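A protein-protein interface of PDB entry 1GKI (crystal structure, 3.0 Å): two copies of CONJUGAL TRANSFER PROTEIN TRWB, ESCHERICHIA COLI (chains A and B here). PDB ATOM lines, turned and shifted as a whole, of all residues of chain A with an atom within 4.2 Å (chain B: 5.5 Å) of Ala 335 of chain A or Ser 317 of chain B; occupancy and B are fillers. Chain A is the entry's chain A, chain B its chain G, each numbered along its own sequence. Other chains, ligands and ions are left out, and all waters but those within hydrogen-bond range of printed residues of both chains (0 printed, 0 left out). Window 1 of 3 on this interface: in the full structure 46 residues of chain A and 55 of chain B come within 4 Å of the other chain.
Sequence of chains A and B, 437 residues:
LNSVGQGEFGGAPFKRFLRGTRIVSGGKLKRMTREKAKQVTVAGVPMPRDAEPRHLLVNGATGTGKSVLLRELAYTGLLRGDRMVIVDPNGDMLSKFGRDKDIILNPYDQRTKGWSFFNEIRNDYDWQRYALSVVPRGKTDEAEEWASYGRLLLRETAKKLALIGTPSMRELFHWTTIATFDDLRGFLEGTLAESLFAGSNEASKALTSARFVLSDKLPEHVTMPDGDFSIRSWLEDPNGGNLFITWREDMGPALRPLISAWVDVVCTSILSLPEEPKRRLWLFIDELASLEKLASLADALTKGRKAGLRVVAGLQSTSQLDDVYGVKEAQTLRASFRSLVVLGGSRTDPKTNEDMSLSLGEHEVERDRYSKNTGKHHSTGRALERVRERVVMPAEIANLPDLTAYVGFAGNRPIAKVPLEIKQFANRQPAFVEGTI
O of Phe 337 of chain A is in hydrogen-bond range of OG1 of Thr 348 of chain B (3.0 Å).
OG of Ser 346 of chain B sits at hydrogen-bond distance from O of Phe 337 of chain A (2.9 Å).
The side-chain hydroxyl (OG) of Ser 319 of chain B sits at hydrogen-bond distance from the side-chain hydroxyl (OG1) of Thr 332 of chain A.
O of Arg 334 of chain A lies within hydrogen-bond range of OG1 of Thr 348 of chain B (2.8 Å).
The side-chain amide nitrogen (NE2) of Gln 331 of chain A lies close to the side-chain carboxylate (OD1) of Asp 349 of chain B (3.5 Å).
The side-chain amide nitrogen (NE2) of Gln 331 of chain A sits at hydrogen-bond distance from the side-chain hydroxyl (OG1) of Thr 352 of chain B (3.4 Å).
OG of Ser 317 of chain B is in hydrogen-bond range of OD2 of Asp 349 of chain B, 3.4 Å away.
OG of Ser 336 of chain A sits at hydrogen-bond distance from O of Thr 332 of chain A (3.0 Å).
OE1 of Gln 320 of chain B sits at hydrogen-bond distance from N of Ser 317 of chain B (3.4 Å).
The side-chain hydroxyl (OG) of Ser 346 of chain B is in hydrogen-bond range of the side-chain hydroxyl (OG1) of Thr 348 of chain B.
OD2 of Asp 349 of chain B lies within hydrogen-bond range of OG1 of Thr 352 of chain B, 2.4 Å away.
Ser 319 of chain B touches Gln 331 of chain A.
Thr 332 of chain A touches Gln 320 of chain B (CG2 to CG, 3.5 Å).
CB of Ala 335 of chain A touches OG of Ser 317 of chain B, 3.5 Å away.
Ser 346 of chain B touches Ala 335 of chain A (CB to O, 3.4 Å).
OG1 of Thr 348 of chain B touches CA of Ala 335 of chain A (3.7 Å).
CB of Asp 349 of chain B touches CB of Ala 335 of chain A (3.5 Å).
Ala 335 of chain A touches just these residues of chain B: Ser 317 (3.5 Å), Ser 346 (3.4 Å), Thr 348 (3.7 Å) and Asp 349 (3.5 Å).
Printed residues of chain A within 4 Å of Ser 317 of chain B: Ala 335.
Printed residues of chain A within 4 Å of Asp 349 of chain B: Gln 331 and Ala 335.
Of the printed residues of chain B, Gln 331 of chain A touches Ser 319, Asp 349 and Thr 352.
Printed residues of chain B within 4 Å of Arg 334 of chain A: Thr 348.
Leu 333 of chain A touches none of the printed residues of chain B.
The nearest residue of chain B that does not touch Ala 335 of chain A is Thr 62 of chain B (5.1 Å).
The nearest printed residue of chain A that does not touch Ser 317 of chain B is Thr 332 of chain A (4.02 Å).
The nearest printed residue of chain B that does not touch Arg 334 of chain A is Ser 346 of chain B (4.7 Å).
No position is printed for both chains.
Of the 12 pairs that touch across the chains among the printed residues, none has its exchanged pair printed and touching as well.
Hydrophobic or aromatic side chains of chain A that line the printed part of chain B: Ala 335.
Among the printed residues, no Asp or Glu carboxylate lies within 4 Å of a Lys or Arg side-chain nitrogen of the other chain.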
ATOM      1  N   GLN A 331      21.692 -13.266  22.421  1.00  0.00           N
ATOM      2  CA  GLN A 331      22.825 -13.503  23.313  1.00  0.00           C
ATOM      3  C   GLN A 331      24.069 -13.687  22.459  1.00  0.00           C
ATOM      4  O   GLN A 331      25.113 -13.104  22.723  1.00  0.00           O
ATOM      5  CB  GLN A 331      22.604 -14.765  24.161  1.00  0.00           C
ATOM      6  CG  GLN A 331      23.713 -15.054  25.178  1.00  0.00           C
ATOM      7  CD  GLN A 331      23.468 -16.328  25.977  1.00  0.00           C
ATOM      8  OE1 GLN A 331      22.353 -16.577  26.440  1.00  0.00           O
ATOM      9  NE2 GLN A 331      24.512 -17.134  26.151  1.00  0.00           N
ATOM     10  N   THR A 332      23.943 -14.500  21.423  1.00  0.00           N
ATOM     11  CA  THR A 332      25.051 -14.761  20.520  1.00  0.00           C
ATOM     12  C   THR A 332      25.493 -13.477  19.835  1.00  0.00           C
ATOM     13  O   THR A 332      26.687 -13.239  19.643  1.00  0.00           O
ATOM     14  CB  THR A 332      24.639 -15.772  19.444  1.00  0.00           C
ATOM     15  OG1 THR A 332      24.200 -16.980  20.079  1.00  0.00           O
ATOM     16  CG2 THR A 332      25.808 -16.072  18.507  1.00  0.00           C
ATOM     17  N   LEU A 333      24.518 -12.656  19.459  1.00  0.00           N
ATOM     18  CA  LEU A 333      24.795 -11.396  18.786  1.00  0.00           C
ATOM     19  C   LEU A 333      25.632 -10.513  19.700  1.00  0.00           C
ATOM     20  O   LEU A 333      26.711 -10.070  19.321  1.00  0.00           O
ATOM     21  CB  LEU A 333      23.486 -10.694  18.425  1.00  0.00           C
ATOM     22  CG  LEU A 333      23.605  -9.477  17.515  1.00  0.00           C
ATOM     23  CD1 LEU A 333      24.298  -9.886  16.235  1.00  0.00           C
ATOM     24  CD2 LEU A 333      22.239  -8.902  17.218  1.00  0.00           C
ATOM     25  N   ARG A 334      25.138 -10.268  20.908  1.00  0.00           N
ATOM     26  CA  ARG A 334      25.867  -9.455  21.869  1.00  0.00           C
ATOM     27  C   ARG A 334      27.252 -10.024  22.155  1.00  0.00           C
ATOM     28  O   ARG A 334      28.228  -9.292  22.211  1.00  0.00           O
ATOM     29  CB  ARG A 334      25.090  -9.348  23.184  1.00  0.00           C
ATOM     30  CG  ARG A 334      23.943  -8.362  23.146  1.00  0.00           C
ATOM     31  CD  ARG A 334      23.340  -8.170  24.522  1.00  0.00           C
ATOM     32  NE  ARG A 334      22.630  -9.354  24.982  1.00  0.00           N
ATOM     33  CZ  ARG A 334      21.314  -9.544  24.880  1.00  0.00           C
ATOM     34  NH1 ARG A 334      20.784 -10.671  25.331  1.00  0.00           N
ATOM     35  NH2 ARG A 334      20.524  -8.617  24.351  1.00  0.00           N
ATOM     36  N   ALA A 335      27.335 -11.333  22.332  1.00  0.00           N
ATOM     37  CA  ALA A 335      28.608 -11.975  22.628  1.00  0.00           C
ATOM     38  C   ALA A 335      29.665 -11.733  21.548  1.00  0.00           C
ATOM     39  O   ALA A 335      30.863 -11.902  21.797  1.00  0.00           O
ATOM     40  CB  ALA A 335      28.395 -13.473  22.823  1.00  0.00           C
ATOM     41  N   SER A 336      29.220 -11.339  20.354  1.00  0.00           N
ATOM     42  CA  SER A 336      30.129 -11.090  19.236  1.00  0.00           C
ATOM     43  C   SER A 336      30.847  -9.753  19.328  1.00  0.00           C
ATOM     44  O   SER A 336      31.824  -9.533  18.623  1.00  0.00           O
ATOM     45  CB  SER A 336      29.377 -11.183  17.908  1.00  0.00           C
ATOM     46  OG  SER A 336      28.858 -12.491  17.715  1.00  0.00           O
ATOM     47  N   PHE A 337      30.350  -8.862  20.184  1.00  0.00           N
ATOM     48  CA  PHE A 337      30.975  -7.557  20.408  1.00  0.00           C
ATOM     49  C   PHE A 337      31.886  -7.715  21.630  1.00  0.00           C
ATOM     50  O   PHE A 337      31.405  -7.744  22.762  1.00  0.00           O
ATOM     51  CB  PHE A 337      29.924  -6.482  20.708  1.00  0.00           C
ATOM     52  CG  PHE A 337      28.993  -6.187  19.561  1.00  0.00           C
ATOM     53  CD1 PHE A 337      27.994  -7.087  19.204  1.00  0.00           C
ATOM     54  CD2 PHE A 337      29.105  -5.000  18.846  1.00  0.00           C
ATOM     55  CE1 PHE A 337      27.121  -6.807  18.158  1.00  0.00           C
ATOM     56  CE2 PHE A 337      28.235  -4.712  17.798  1.00  0.00           C
ATOM     57  CZ  PHE A 337      27.244  -5.616  17.456  1.00  0.00           C
ATOM     58  N   ASN B  59      35.725 -24.210  23.539  1.00  0.00           N
ATOM     59  CA  ASN B  59      34.837 -23.056  23.626  1.00  0.00           C
ATOM     60  C   ASN B  59      35.645 -21.768  23.763  1.00  0.00           C
ATOM     61  O   ASN B  59      36.565 -21.693  24.578  1.00  0.00           O
ATOM     62  CB  ASN B  59      33.900 -23.220  24.833  1.00  0.00           C
ATOM     63  CG  ASN B  59      32.742 -22.211  24.832  1.00  0.00           C
ATOM     64  OD1 ASN B  59      31.838 -22.269  23.986  1.00  0.00           O
ATOM     65  ND2 ASN B  59      32.771 -21.281  25.783  1.00  0.00           N
ATOM     66  N   ALA B  61      35.548 -17.165  22.670  1.00  0.00           N
ATOM     67  CA  ALA B  61      35.048 -16.004  21.946  1.00  0.00           C
ATOM     68  C   ALA B  61      35.726 -15.864  20.595  1.00  0.00           C
ATOM     69  O   ALA B  61      36.801 -16.417  20.370  1.00  0.00           O
ATOM     70  CB  ALA B  61      35.271 -14.745  22.767  1.00  0.00           C
ATOM     71  N   THR B  62      35.090 -15.114  19.702  1.00  0.00           N
ATOM     72  CA  THR B  62      35.626 -14.897  18.367  1.00  0.00           C
ATOM     73  C   THR B  62      36.976 -14.187  18.443  1.00  0.00           C
ATOM     74  O   THR B  62      37.108 -13.144  19.084  1.00  0.00           O
ATOM     75  CB  THR B  62      34.619 -14.076  17.484  1.00  0.00           C
ATOM     76  OG1 THR B  62      35.176 -13.861  16.183  1.00  0.00           O
ATOM     77  CG2 THR B  62      34.291 -12.727  18.121  1.00  0.00           C
ATOM     78  N   ALA B 289      28.213 -25.105  15.886  1.00  0.00           N
ATOM     79  CA  ALA B 289      26.937 -24.407  15.781  1.00  0.00           C
ATOM     80  C   ALA B 289      26.579 -23.930  14.381  1.00  0.00           C
ATOM     81  O   ALA B 289      25.430 -23.561  14.127  1.00  0.00           O
ATOM     82  CB  ALA B 289      26.912 -23.235  16.747  1.00  0.00           C
ATOM     83  N   LEU B 315      33.448 -23.935  19.382  1.00  0.00           N
ATOM     84  CA  LEU B 315      32.158 -23.401  19.787  1.00  0.00           C
ATOM     85  C   LEU B 315      32.358 -22.011  20.370  1.00  0.00           C
ATOM     86  O   LEU B 315      33.293 -21.799  21.136  1.00  0.00           O
ATOM     87  CB  LEU B 315      31.553 -24.330  20.842  1.00  0.00           C
ATOM     88  CG  LEU B 315      30.044 -24.370  21.067  1.00  0.00           C
ATOM     89  CD1 LEU B 315      29.309 -24.647  19.757  1.00  0.00           C
ATOM     90  CD2 LEU B 315      29.745 -25.453  22.080  1.00  0.00           C
ATOM     91  N   GLN B 316      31.499 -21.062  20.013  1.00  0.00           N
ATOM     92  CA  GLN B 316      31.631 -19.712  20.557  1.00  0.00           C
ATOM     93  C   GLN B 316      30.686 -19.471  21.724  1.00  0.00           C
ATOM     94  O   GLN B 316      31.137 -19.280  22.853  1.00  0.00           O
ATOM     95  CB  GLN B 316      31.399 -18.676  19.471  1.00  0.00           C
ATOM     96  CG  GLN B 316      32.512 -18.652  18.453  1.00  0.00           C
ATOM     97  CD  GLN B 316      32.227 -17.679  17.341  1.00  0.00           C
ATOM     98  OE1 GLN B 316      33.016 -16.766  17.077  1.00  0.00           O
ATOM     99  NE2 GLN B 316      31.086 -17.861  16.675  1.00  0.00           N
ATOM    100  N   SER B 317      29.380 -19.477  21.454  1.00  0.00           N
ATOM    101  CA  SER B 317      28.376 -19.288  22.506  1.00  0.00           C
ATOM    102  C   SER B 317      27.547 -20.558  22.706  1.00  0.00           C
ATOM    103  O   SER B 317      27.215 -21.266  21.746  1.00  0.00           O
ATOM    104  CB  SER B 317      27.435 -18.119  22.172  1.00  0.00           C
ATOM    105  OG  SER B 317      27.773 -16.954  22.909  1.00  0.00           O
ATOM    106  N   THR B 318      27.230 -20.851  23.961  1.00  0.00           N
ATOM    107  CA  THR B 318      26.437 -22.026  24.260  1.00  0.00           C
ATOM    108  C   THR B 318      25.036 -21.741  23.750  1.00  0.00           C
ATOM    109  O   THR B 318      24.272 -22.657  23.454  1.00  0.00           O
ATOM    110  CB  THR B 318      26.393 -22.312  25.778  1.00  0.00           C
ATOM    111  OG1 THR B 318      26.130 -21.094  26.490  1.00  0.00           O
ATOM    112  CG2 THR B 318      27.712 -22.916  26.242  1.00  0.00           C
ATOM    113  N   SER B 319      24.710 -20.458  23.634  1.00  0.00           N
ATOM    114  CA  SER B 319      23.395 -20.057  23.152  1.00  0.00           C
ATOM    115  C   SER B 319      23.183 -20.471  21.701  1.00  0.00           C
ATOM    116  O   SER B 319      22.047 -20.657  21.269  1.00  0.00           O
ATOM    117  CB  SER B 319      23.207 -18.542  23.299  1.00  0.00           C
ATOM    118  OG  SER B 319      24.261 -17.822  22.684  1.00  0.00           O
ATOM    119  N   GLN B 320      24.271 -20.610  20.948  1.00  0.00           N
ATOM    120  CA  GLN B 320      24.171 -21.026  19.553  1.00  0.00           C
ATOM    121  C   GLN B 320      23.703 -22.473  19.482  1.00  0.00           C
ATOM    122  O   GLN B 320      22.639 -22.766  18.940  1.00  0.00           O
ATOM    123  CB  GLN B 320      25.522 -20.947  18.858  1.00  0.00           C
ATOM    124  CG  GLN B 320      25.925 -19.600  18.327  1.00  0.00           C
ATOM    125  CD  GLN B 320      27.279 -19.666  17.621  1.00  0.00           C
ATOM    126  OE1 GLN B 320      28.315 -19.951  18.250  1.00  0.00           O
ATOM    127  NE2 GLN B 320      27.276 -19.422  16.306  1.00  0.00           N
ATOM    128  N   LEU B 321      24.514 -23.374  20.027  1.00  0.00           N
ATOM    129  CA  LEU B 321      24.196 -24.791  20.021  1.00  0.00           C
ATOM    130  C   LEU B 321      22.762 -24.993  20.484  1.00  0.00           C
ATOM    131  O   LEU B 321      22.028 -25.796  19.916  1.00  0.00           O
ATOM    132  CB  LEU B 321      25.156 -25.540  20.940  1.00  0.00           C
ATOM    133  CG  LEU B 321      25.308 -27.038  20.695  1.00  0.00           C
ATOM    134  CD1 LEU B 321      25.835 -27.258  19.295  1.00  0.00           C
ATOM    135  CD2 LEU B 321      26.253 -27.639  21.724  1.00  0.00           C
ATOM    136  N   SER B 346      33.736 -12.891  25.664  1.00  0.00           N
ATOM    137  CA  SER B 346      33.451 -11.474  25.773  1.00  0.00           C
ATOM    138  C   SER B 346      32.760 -11.130  27.090  1.00  0.00           C
ATOM    139  O   SER B 346      32.062 -11.960  27.663  1.00  0.00           O
ATOM    140  CB  SER B 346      32.577 -11.038  24.599  1.00  0.00           C
ATOM    141  OG  SER B 346      32.180  -9.685  24.745  1.00  0.00           O
ATOM    142  N   THR B 348      30.495  -8.952  27.339  1.00  0.00           N
ATOM    143  CA  THR B 348      29.129  -8.554  27.036  1.00  0.00           C
ATOM    144  C   THR B 348      28.207  -9.763  27.168  1.00  0.00           C
ATOM    145  O   THR B 348      26.984  -9.637  27.094  1.00  0.00           O
ATOM    146  CB  THR B 348      29.009  -8.004  25.613  1.00  0.00           C
ATOM    147  OG1 THR B 348      29.420  -9.008  24.680  1.00  0.00           O
ATOM    148  CG2 THR B 348      29.883  -6.781  25.443  1.00  0.00           C
ATOM    149  N   ASP B 349      28.806 -10.933  27.368  1.00  0.00           N
ATOM    150  CA  ASP B 349      28.050 -12.170  27.515  1.00  0.00           C
ATOM    151  C   ASP B 349      28.407 -12.896  28.816  1.00  0.00           C
ATOM    152  O   ASP B 349      29.102 -13.916  28.809  1.00  0.00           O
ATOM    153  CB  ASP B 349      28.308 -13.076  26.311  1.00  0.00           C
ATOM    154  CG  ASP B 349      27.621 -14.418  26.432  1.00  0.00           C
ATOM    155  OD1 ASP B 349      26.537 -14.470  27.060  1.00  0.00           O
ATOM    156  OD2 ASP B 349      28.159 -15.409  25.887  1.00  0.00           O
ATOM    157  N   THR B 352      27.539 -17.043  29.314  1.00  0.00           N
ATOM    158  CA  THR B 352      28.502 -18.032  28.888  1.00  0.00           C
ATOM    159  C   THR B 352      29.676 -18.066  29.868  1.00  0.00           C
ATOM    160  O   THR B 352      30.130 -19.140  30.252  1.00  0.00           O
ATOM    161  CB  THR B 352      28.998 -17.730  27.472  1.00  0.00           C
ATOM    162  OG1 THR B 352      27.883 -17.718  26.578  1.00  0.00           O
ATOM    163  CG2 THR B 352      29.967 -18.795  27.009  1.00  0.00           C
